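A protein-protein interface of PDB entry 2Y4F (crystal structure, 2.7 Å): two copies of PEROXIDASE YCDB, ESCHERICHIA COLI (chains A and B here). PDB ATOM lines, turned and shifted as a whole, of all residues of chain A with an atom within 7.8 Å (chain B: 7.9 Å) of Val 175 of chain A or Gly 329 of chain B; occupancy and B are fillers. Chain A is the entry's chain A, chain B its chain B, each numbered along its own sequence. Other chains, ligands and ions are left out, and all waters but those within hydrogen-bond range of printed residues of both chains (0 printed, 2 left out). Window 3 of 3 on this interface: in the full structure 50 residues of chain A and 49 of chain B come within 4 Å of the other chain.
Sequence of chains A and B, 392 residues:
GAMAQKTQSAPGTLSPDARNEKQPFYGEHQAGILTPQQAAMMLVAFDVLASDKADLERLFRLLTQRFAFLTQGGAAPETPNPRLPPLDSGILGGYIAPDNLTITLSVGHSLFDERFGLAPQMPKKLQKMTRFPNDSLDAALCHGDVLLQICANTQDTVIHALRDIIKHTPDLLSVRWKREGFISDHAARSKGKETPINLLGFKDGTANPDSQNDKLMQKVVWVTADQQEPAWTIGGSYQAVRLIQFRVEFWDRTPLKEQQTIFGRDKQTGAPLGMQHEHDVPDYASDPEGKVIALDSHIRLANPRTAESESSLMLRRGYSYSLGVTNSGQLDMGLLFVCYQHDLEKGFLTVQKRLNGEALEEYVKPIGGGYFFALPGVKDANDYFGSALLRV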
ATOM      1  N   LEU A  43     -12.124 -22.278 -16.882  1.00  0.00           N
ATOM      2  CA  LEU A  43     -11.160 -21.714 -17.803  1.00  0.00           C
ATOM      3  C   LEU A  43     -11.449 -22.318 -19.165  1.00  0.00           C
ATOM      4  O   LEU A  43     -11.412 -23.538 -19.331  1.00  0.00           O
ATOM      5  CB  LEU A  43      -9.763 -22.081 -17.360  1.00  0.00           C
ATOM      6  CG  LEU A  43      -9.341 -21.499 -16.018  1.00  0.00           C
ATOM      7  CD1 LEU A  43      -7.959 -22.026 -15.612  1.00  0.00           C
ATOM      8  CD2 LEU A  43      -9.371 -19.983 -16.035  1.00  0.00           C
ATOM      9  N   VAL A  44     -11.775 -21.487 -20.138  1.00  0.00           N
ATOM     10  CA  VAL A  44     -12.100 -22.017 -21.435  1.00  0.00           C
ATOM     11  C   VAL A  44     -11.403 -21.174 -22.496  1.00  0.00           C
ATOM     12  O   VAL A  44     -11.568 -19.958 -22.554  1.00  0.00           O
ATOM     13  CB  VAL A  44     -13.652 -22.186 -21.614  1.00  0.00           C
ATOM     14  CG1 VAL A  44     -14.407 -20.895 -21.287  1.00  0.00           C
ATOM     15  CG2 VAL A  44     -14.000 -22.710 -22.982  1.00  0.00           C
ATOM     16  N   ALA A  45     -10.558 -21.841 -23.278  1.00  0.00           N
ATOM     17  CA  ALA A  45      -9.820 -21.228 -24.374  1.00  0.00           C
ATOM     18  C   ALA A  45     -10.589 -21.468 -25.669  1.00  0.00           C
ATOM     19  O   ALA A  45     -11.192 -22.542 -25.847  1.00  0.00           O
ATOM     20  CB  ALA A  45      -8.428 -21.818 -24.459  1.00  0.00           C
ATOM     21  N   PHE A  46     -10.596 -20.462 -26.545  1.00  0.00           N
ATOM     22  CA  PHE A  46     -11.212 -20.581 -27.871  1.00  0.00           C
ATOM     23  C   PHE A  46     -10.217 -20.292 -28.982  1.00  0.00           C
ATOM     24  O   PHE A  46      -9.318 -19.447 -28.838  1.00  0.00           O
ATOM     25  CB  PHE A  46     -12.385 -19.617 -28.043  1.00  0.00           C
ATOM     26  CG  PHE A  46     -13.566 -19.958 -27.217  1.00  0.00           C
ATOM     27  CD1 PHE A  46     -14.511 -20.861 -27.679  1.00  0.00           C
ATOM     28  CD2 PHE A  46     -13.741 -19.383 -25.974  1.00  0.00           C
ATOM     29  CE1 PHE A  46     -15.631 -21.188 -26.904  1.00  0.00           C
ATOM     30  CE2 PHE A  46     -14.844 -19.706 -25.199  1.00  0.00           C
ATOM     31  CZ  PHE A  46     -15.795 -20.613 -25.668  1.00  0.00           C
ATOM     32  N   ASP A  47     -10.374 -21.012 -30.087  1.00  0.00           N
ATOM     33  CA  ASP A  47      -9.786 -20.574 -31.323  1.00  0.00           C
ATOM     34  C   ASP A  47     -10.815 -19.595 -31.872  1.00  0.00           C
ATOM     35  O   ASP A  47     -12.015 -19.915 -31.980  1.00  0.00           O
ATOM     36  CB  ASP A  47      -9.581 -21.731 -32.320  1.00  0.00           C
ATOM     37  CG  ASP A  47      -8.756 -22.885 -31.759  1.00  0.00           C
ATOM     38  OD1 ASP A  47      -7.754 -22.650 -31.047  1.00  0.00           O
ATOM     39  OD2 ASP A  47      -9.126 -24.046 -32.052  1.00  0.00           O
ATOM     40  N   VAL A  48     -10.342 -18.395 -32.185  1.00  0.00           N
ATOM     41  CA  VAL A  48     -11.147 -17.420 -32.897  1.00  0.00           C
ATOM     42  C   VAL A  48     -11.261 -17.828 -34.369  1.00  0.00           C
ATOM     43  O   VAL A  48     -10.251 -18.140 -35.015  1.00  0.00           O
ATOM     44  CB  VAL A  48     -10.552 -16.017 -32.758  1.00  0.00           C
ATOM     45  CG1 VAL A  48     -10.956 -15.146 -33.910  1.00  0.00           C
ATOM     46  CG2 VAL A  48     -10.988 -15.393 -31.443  1.00  0.00           C
ATOM     47  N   LEU A  49     -12.496 -17.850 -34.873  1.00  0.00           N
ATOM     48  CA  LEU A  49     -12.773 -18.175 -36.272  1.00  0.00           C
ATOM     49  C   LEU A  49     -13.063 -16.948 -37.128  1.00  0.00           C
ATOM     50  O   LEU A  49     -13.363 -17.086 -38.310  1.00  0.00           O
ATOM     51  CB  LEU A  49     -13.948 -19.136 -36.385  1.00  0.00           C
ATOM     52  CG  LEU A  49     -13.886 -20.316 -35.432  1.00  0.00           C
ATOM     53  CD1 LEU A  49     -15.181 -21.156 -35.528  1.00  0.00           C
ATOM     54  CD2 LEU A  49     -12.611 -21.152 -35.677  1.00  0.00           C
ATOM     55  N   ALA A 140      -2.886 -30.077 -26.263  1.00  0.00           N
ATOM     56  CA  ALA A 140      -4.340 -29.956 -26.242  1.00  0.00           C
ATOM     57  C   ALA A 140      -4.793 -29.005 -25.139  1.00  0.00           C
ATOM     58  O   ALA A 140      -5.883 -28.441 -25.220  1.00  0.00           O
ATOM     59  CB  ALA A 140      -5.005 -31.338 -26.082  1.00  0.00           C
ATOM     60  N   LEU A 162     -21.422 -20.515 -20.389  1.00  0.00           N
ATOM     61  CA  LEU A 162     -20.657 -21.109 -21.473  1.00  0.00           C
ATOM     62  C   LEU A 162     -21.495 -21.525 -22.682  1.00  0.00           C
ATOM     63  O   LEU A 162     -21.218 -21.129 -23.828  1.00  0.00           O
ATOM     64  CB  LEU A 162     -19.879 -22.321 -20.971  1.00  0.00           C
ATOM     65  CG  LEU A 162     -19.042 -23.070 -22.013  1.00  0.00           C
ATOM     66  CD1 LEU A 162     -18.005 -22.137 -22.615  1.00  0.00           C
ATOM     67  CD2 LEU A 162     -18.392 -24.293 -21.400  1.00  0.00           C
ATOM     68  N   ILE A 166     -21.505 -20.091 -26.444  1.00  0.00           N
ATOM     69  CA  ILE A 166     -21.239 -20.970 -27.569  1.00  0.00           C
ATOM     70  C   ILE A 166     -22.361 -20.880 -28.595  1.00  0.00           C
ATOM     71  O   ILE A 166     -22.113 -20.579 -29.772  1.00  0.00           O
ATOM     72  CB  ILE A 166     -21.048 -22.415 -27.095  1.00  0.00           C
ATOM     73  CG1 ILE A 166     -19.600 -22.618 -26.636  1.00  0.00           C
ATOM     74  CG2 ILE A 166     -21.393 -23.390 -28.193  1.00  0.00           C
ATOM     75  CD1 ILE A 166     -19.415 -23.794 -25.691  1.00  0.00           C
ATOM     76  N   THR A 169     -22.182 -18.137 -30.945  1.00  0.00           N
ATOM     77  CA  THR A 169     -20.910 -17.864 -31.644  1.00  0.00           C
ATOM     78  C   THR A 169     -20.437 -18.901 -32.678  1.00  0.00           C
ATOM     79  O   THR A 169     -19.242 -18.945 -32.988  1.00  0.00           O
ATOM     80  CB  THR A 169     -19.732 -17.580 -30.640  1.00  0.00           C
ATOM     81  OG1 THR A 169     -19.649 -18.627 -29.664  1.00  0.00           O
ATOM     82  CG2 THR A 169     -19.901 -16.230 -29.939  1.00  0.00           C
ATOM     83  N   LEU A 173     -16.381 -18.646 -32.752  1.00  0.00           N
ATOM     84  CA  LEU A 173     -15.605 -19.346 -31.709  1.00  0.00           C
ATOM     85  C   LEU A 173     -15.535 -20.893 -31.813  1.00  0.00           C
ATOM     86  O   LEU A 173     -16.492 -21.560 -32.237  1.00  0.00           O
ATOM     87  CB  LEU A 173     -16.143 -18.992 -30.325  1.00  0.00           C
ATOM     88  CG  LEU A 173     -15.935 -17.598 -29.756  1.00  0.00           C
ATOM     89  CD1 LEU A 173     -16.238 -17.681 -28.282  1.00  0.00           C
ATOM     90  CD2 LEU A 173     -14.514 -17.050 -30.000  1.00  0.00           C
ATOM     91  N   SER A 174     -14.406 -21.457 -31.383  1.00  0.00           N
ATOM     92  CA  SER A 174     -14.243 -22.902 -31.344  1.00  0.00           C
ATOM     93  C   SER A 174     -13.533 -23.281 -30.070  1.00  0.00           C
ATOM     94  O   SER A 174     -12.412 -22.824 -29.830  1.00  0.00           O
ATOM     95  CB  SER A 174     -13.433 -23.380 -32.549  1.00  0.00           C
ATOM     96  OG  SER A 174     -13.623 -24.767 -32.752  1.00  0.00           O
ATOM     97  N   VAL A 175     -14.195 -24.101 -29.261  1.00  0.00           N
ATOM     98  CA  VAL A 175     -13.695 -24.509 -27.953  1.00  0.00           C
ATOM     99  C   VAL A 175     -12.372 -25.187 -28.178  1.00  0.00           C
ATOM    100  O   VAL A 175     -12.318 -26.206 -28.849  1.00  0.00           O
ATOM    101  CB  VAL A 175     -14.683 -25.511 -27.233  1.00  0.00           C
ATOM    102  CG1 VAL A 175     -14.048 -26.164 -26.037  1.00  0.00           C
ATOM    103  CG2 VAL A 175     -15.934 -24.789 -26.781  1.00  0.00           C
ATOM    104  N   ARG A 176     -11.307 -24.599 -27.648  1.00  0.00           N
ATOM    105  CA  ARG A 176      -9.973 -25.170 -27.720  1.00  0.00           C
ATOM    106  C   ARG A 176      -9.814 -26.166 -26.568  1.00  0.00           C
ATOM    107  O   ARG A 176     -10.111 -27.339 -26.746  1.00  0.00           O
ATOM    108  CB  ARG A 176      -8.922 -24.059 -27.704  1.00  0.00           C
ATOM    109  CG  ARG A 176      -7.498 -24.549 -27.883  1.00  0.00           C
ATOM    110  CD  ARG A 176      -6.502 -23.421 -27.865  1.00  0.00           C
ATOM    111  NE  ARG A 176      -5.137 -23.925 -28.008  1.00  0.00           N
ATOM    112  CZ  ARG A 176      -4.477 -24.035 -29.166  1.00  0.00           C
ATOM    113  NH1 ARG A 176      -5.048 -23.663 -30.311  1.00  0.00           N
ATOM    114  NH2 ARG A 176      -3.236 -24.509 -29.171  1.00  0.00           N
ATOM    115  N   TRP A 177      -9.384 -25.715 -25.388  1.00  0.00           N
ATOM    116  CA  TRP A 177      -9.415 -26.568 -24.181  1.00  0.00           C
ATOM    117  C   TRP A 177     -10.372 -26.009 -23.152  1.00  0.00           C
ATOM    118  O   TRP A 177     -10.670 -24.811 -23.177  1.00  0.00           O
ATOM    119  CB  TRP A 177      -8.034 -26.724 -23.542  1.00  0.00           C
ATOM    120  CG  TRP A 177      -7.260 -25.450 -23.342  1.00  0.00           C
ATOM    121  CD1 TRP A 177      -6.516 -24.787 -24.288  1.00  0.00           C
ATOM    122  CD2 TRP A 177      -7.108 -24.702 -22.131  1.00  0.00           C
ATOM    123  NE1 TRP A 177      -5.918 -23.676 -23.737  1.00  0.00           N
ATOM    124  CE2 TRP A 177      -6.272 -23.601 -22.415  1.00  0.00           C
ATOM    125  CE3 TRP A 177      -7.606 -24.838 -20.841  1.00  0.00           C
ATOM    126  CZ2 TRP A 177      -5.920 -22.650 -21.442  1.00  0.00           C
ATOM    127  CZ3 TRP A 177      -7.244 -23.879 -19.863  1.00  0.00           C
ATOM    128  CH2 TRP A 177      -6.414 -22.815 -20.177  1.00  0.00           C
ATOM    129  N   LYS A 178     -10.831 -26.867 -22.243  1.00  0.00           N
ATOM    130  CA  LYS A 178     -11.635 -26.425 -21.115  1.00  0.00           C
ATOM    131  C   LYS A 178     -11.358 -27.196 -19.819  1.00  0.00           C
ATOM    132  O   LYS A 178     -11.291 -28.425 -19.834  1.00  0.00           O
ATOM    133  CB  LYS A 178     -13.119 -26.505 -21.466  1.00  0.00           C
ATOM    134  CG  LYS A 178     -14.065 -26.233 -20.307  1.00  0.00           C
ATOM    135  CD  LYS A 178     -15.143 -27.303 -20.297  1.00  0.00           C
ATOM    136  CE  LYS A 178     -16.035 -27.168 -19.093  1.00  0.00           C
ATOM    137  NZ  LYS A 178     -16.680 -28.466 -18.711  1.00  0.00           N
ATOM    138  N   GLU B 249     -23.719 -29.136 -27.752  1.00  0.00           N
ATOM    139  CA  GLU B 249     -23.827 -28.018 -28.687  1.00  0.00           C
ATOM    140  C   GLU B 249     -24.870 -28.346 -29.762  1.00  0.00           C
ATOM    141  O   GLU B 249     -25.699 -27.499 -30.141  1.00  0.00           O
ATOM    142  CB  GLU B 249     -22.479 -27.735 -29.354  1.00  0.00           C
ATOM    143  CG  GLU B 249     -21.327 -27.524 -28.405  1.00  0.00           C
ATOM    144  CD  GLU B 249     -20.538 -28.796 -28.085  1.00  0.00           C
ATOM    145  OE1 GLU B 249     -21.090 -29.902 -28.160  1.00  0.00           O
ATOM    146  OE2 GLU B 249     -19.344 -28.670 -27.736  1.00  0.00           O
ATOM    147  N   GLY B 324     -14.205 -31.950 -19.513  1.00  0.00           N
ATOM    148  CA  GLY B 324     -13.409 -31.082 -20.372  1.00  0.00           C
ATOM    149  C   GLY B 324     -13.882 -31.148 -21.808  1.00  0.00           C
ATOM    150  O   GLY B 324     -15.019 -30.805 -22.114  1.00  0.00           O
ATOM    151  N   VAL B 325     -13.008 -31.609 -22.692  1.00  0.00           N
ATOM    152  CA  VAL B 325     -13.275 -31.587 -24.130  1.00  0.00           C
ATOM    153  C   VAL B 325     -13.122 -33.005 -24.670  1.00  0.00           C
ATOM    154  O   VAL B 325     -12.188 -33.697 -24.275  1.00  0.00           O
ATOM    155  CB  VAL B 325     -12.289 -30.612 -24.835  1.00  0.00           C
ATOM    156  CG1 VAL B 325     -12.342 -30.756 -26.310  1.00  0.00           C
ATOM    157  CG2 VAL B 325     -12.606 -29.176 -24.462  1.00  0.00           C
ATOM    158  N   THR B 326     -14.019 -33.449 -25.553  1.00  0.00           N
ATOM    159  CA  THR B 326     -13.841 -34.757 -26.227  1.00  0.00           C
ATOM    160  C   THR B 326     -12.700 -34.747 -27.258  1.00  0.00           C
ATOM    161  O   THR B 326     -12.229 -33.685 -27.676  1.00  0.00           O
ATOM    162  CB  THR B 326     -15.137 -35.274 -26.915  1.00  0.00           C
ATOM    163  OG1 THR B 326     -15.513 -34.401 -27.991  1.00  0.00           O
ATOM    164  CG2 THR B 326     -16.276 -35.381 -25.914  1.00  0.00           C
ATOM    165  N   ASN B 327     -12.257 -35.945 -27.656  1.00  0.00           N
ATOM    166  CA  ASN B 327     -11.284 -36.112 -28.749  1.00  0.00           C
ATOM    167  C   ASN B 327     -11.764 -35.401 -30.016  1.00  0.00           C
ATOM    168  O   ASN B 327     -10.979 -34.764 -30.739  1.00  0.00           O
ATOM    169  CB  ASN B 327     -11.045 -37.594 -29.042  1.00  0.00           C
ATOM    170  CG  ASN B 327     -10.574 -38.368 -27.817  1.00  0.00           C
ATOM    171  OD1 ASN B 327     -11.384 -38.863 -27.023  1.00  0.00           O
ATOM    172  ND2 ASN B 327      -9.259 -38.490 -27.668  1.00  0.00           N
ATOM    173  N   SER B 328     -13.069 -35.489 -30.257  1.00  0.00           N
ATOM    174  CA  SER B 328     -13.701 -34.774 -31.362  1.00  0.00           C
ATOM    175  C   SER B 328     -13.873 -33.269 -31.110  1.00  0.00           C
ATOM    176  O   SER B 328     -14.549 -32.589 -31.884  1.00  0.00           O
ATOM    177  CB  SER B 328     -15.042 -35.427 -31.709  1.00  0.00           C
ATOM    178  OG  SER B 328     -15.638 -36.016 -30.552  1.00  0.00           O
ATOM    179  N   GLY B 329     -13.258 -32.755 -30.039  1.00  0.00           N
ATOM    180  CA  GLY B 329     -13.194 -31.314 -29.772  1.00  0.00           C
ATOM    181  C   GLY B 329     -14.416 -30.688 -29.115  1.00  0.00           C
ATOM    182  O   GLY B 329     -14.438 -29.485 -28.884  1.00  0.00           O
ATOM    183  N   GLN B 330     -15.432 -31.490 -28.805  1.00  0.00           N
ATOM    184  CA  GLN B 330     -16.673 -30.968 -28.227  1.00  0.00           C
ATOM    185  C   GLN B 330     -16.715 -31.048 -26.693  1.00  0.00           C
ATOM    186  O   GLN B 330     -15.991 -31.846 -26.075  1.00  0.00           O
ATOM    187  CB  GLN B 330     -17.877 -31.722 -28.793  1.00  0.00           C
ATOM    188  CG  GLN B 330     -18.348 -31.254 -30.165  1.00  0.00           C
ATOM    189  CD  GLN B 330     -17.435 -31.728 -31.274  1.00  0.00           C
ATOM    190  OE1 GLN B 330     -17.189 -32.932 -31.415  1.00  0.00           O
ATOM    191  NE2 GLN B 330     -16.914 -30.785 -32.070  1.00  0.00           N
ATOM    192  N   LEU B 331     -17.588 -30.240 -26.090  1.00  0.00           N
ATOM    193  CA  LEU B 331     -17.797 -30.235 -24.642  1.00  0.00           C
ATOM    194  C   LEU B 331     -18.119 -31.614 -24.090  1.00  0.00           C
ATOM    195  O   LEU B 331     -18.901 -32.375 -24.673  1.00  0.00           O
ATOM    196  CB  LEU B 331     -18.923 -29.273 -24.265  1.00  0.00           C
ATOM    197  CG  LEU B 331     -18.659 -27.803 -24.566  1.00  0.00           C
ATOM    198  CD1 LEU B 331     -19.899 -26.995 -24.249  1.00  0.00           C
ATOM    199  CD2 LEU B 331     -17.441 -27.313 -23.778  1.00  0.00           C
ATOM    200  N   ASP B 332     -17.524 -31.938 -22.951  1.00  0.00           N
ATOM    201  CA  ASP B 332     -17.778 -33.243 -22.371  1.00  0.00           C
ATOM    202  C   ASP B 332     -18.647 -33.165 -21.130  1.00  0.00           C
ATOM    203  O   ASP B 332     -18.164 -32.981 -20.015  1.00  0.00           O
ATOM    204  CB  ASP B 332     -16.484 -33.999 -22.117  1.00  0.00           C
ATOM    205  CG  ASP B 332     -16.727 -35.363 -21.563  1.00  0.00           C
ATOM    206  OD1 ASP B 332     -17.824 -35.934 -21.767  1.00  0.00           O
ATOM    207  OD2 ASP B 332     -15.803 -35.862 -20.895  1.00  0.00           O
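The backbone carbonyl oxygen (O) of Ala 45 of chain A lies within hydrogen-bond range of the backbone NH (N) of Arg 176 of chain A, 2.7 Å away.
The guanidinium group (NH1) of Arg 176 of chain A is in salt-bridge range of the side-chain carboxylate (OD1) of Asp 47 of chain A, 3.0 Å away.
OG1 of Thr 169 of chain A is in hydrogen-bond range of O of Ile 166 of chain A, at 3.1 Å.
The side-chain carboxylate (OE2) of Glu 249 of chain B lies within hydrogen-bond range of the backbone NH (N) of Leu 331 of chain B, 2.9 Å away.
O of Gly 324 of chain B lies within hydrogen-bond range of N of Asp 332 of chain B, at 2.9 Å.
The side-chain hydroxyl (OG1) of Thr 326 of chain B is in hydrogen-bond range of the backbone NH (N) of Gly 329 of chain B (3.5 Å).
Among the printed residues, pairs that only touch across the chains: Lys 178 of chain A with Gly 324 of chain B (3.4 Å), Ile 166 of chain A with Leu 331 of chain B (3.5 Å), Lys 178 of chain A with Val 325 of chain B (3.7 Å), Val 175 of chain A with Val 325 of chain B (3.7 Å), Arg 176 of chain A with Val 325 of chain B (3.8 Å), Val 175 of chain A with Gly 329 of chain B (3.9 Å) and Leu 162 of chain A with Leu 331 of chain B (3.96 Å).
Asp 47 of chain A touches none of the printed residues of chain B.
Printed residues of chain B within 4 Å of Ile 166 of chain A: Leu 331.
No residue of chain B comes within 4 Å of Ser 174 of chain A.
Of chain B, only Val 325 (3.7 Å) and Gly 329 (3.9 Å) come within 4 Å of Val 175 of chain A.
Trp 177 of chain A touches none of the printed residues of chain B.
Printed residues of chain B within 4 Å of Lys 178 of chain A: Gly 324 and Val 325.
Gly 329 of chain B touches just one residue of chain A: Val 175 (3.9 Å).
Of the printed residues of chain A, Leu 331 of chain B touches Leu 162 (3.96 Å) and Ile 166 (3.5 Å).
The nearest residue of chain B that does not touch Val 175 of chain A is Leu 331 of chain B (4.2 Å).
The nearest printed residue of chain A that does not touch Val 325 of chain B is Trp 177 of chain A (4.1 Å).
Hydrophobic or aromatic side chains of chain A within 4 Å of the printed part of chain B: Leu 162, Ile 166 and Val 175.
Along chain A the printed residues that touch a printed residue of chain B span positions 162 to 178.
Among the printed residues, 7 pairs touch across the chains.
Among the printed residues, no Asp or Glu carboxylate lies within 4 Å of a Lys or Arg side-chain nitrogen of the other chain.
No position is printed for both chains.
Of the 7 pairs that touch across the chains among the printed residues, none has its exchanged pair printed and touching as well.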
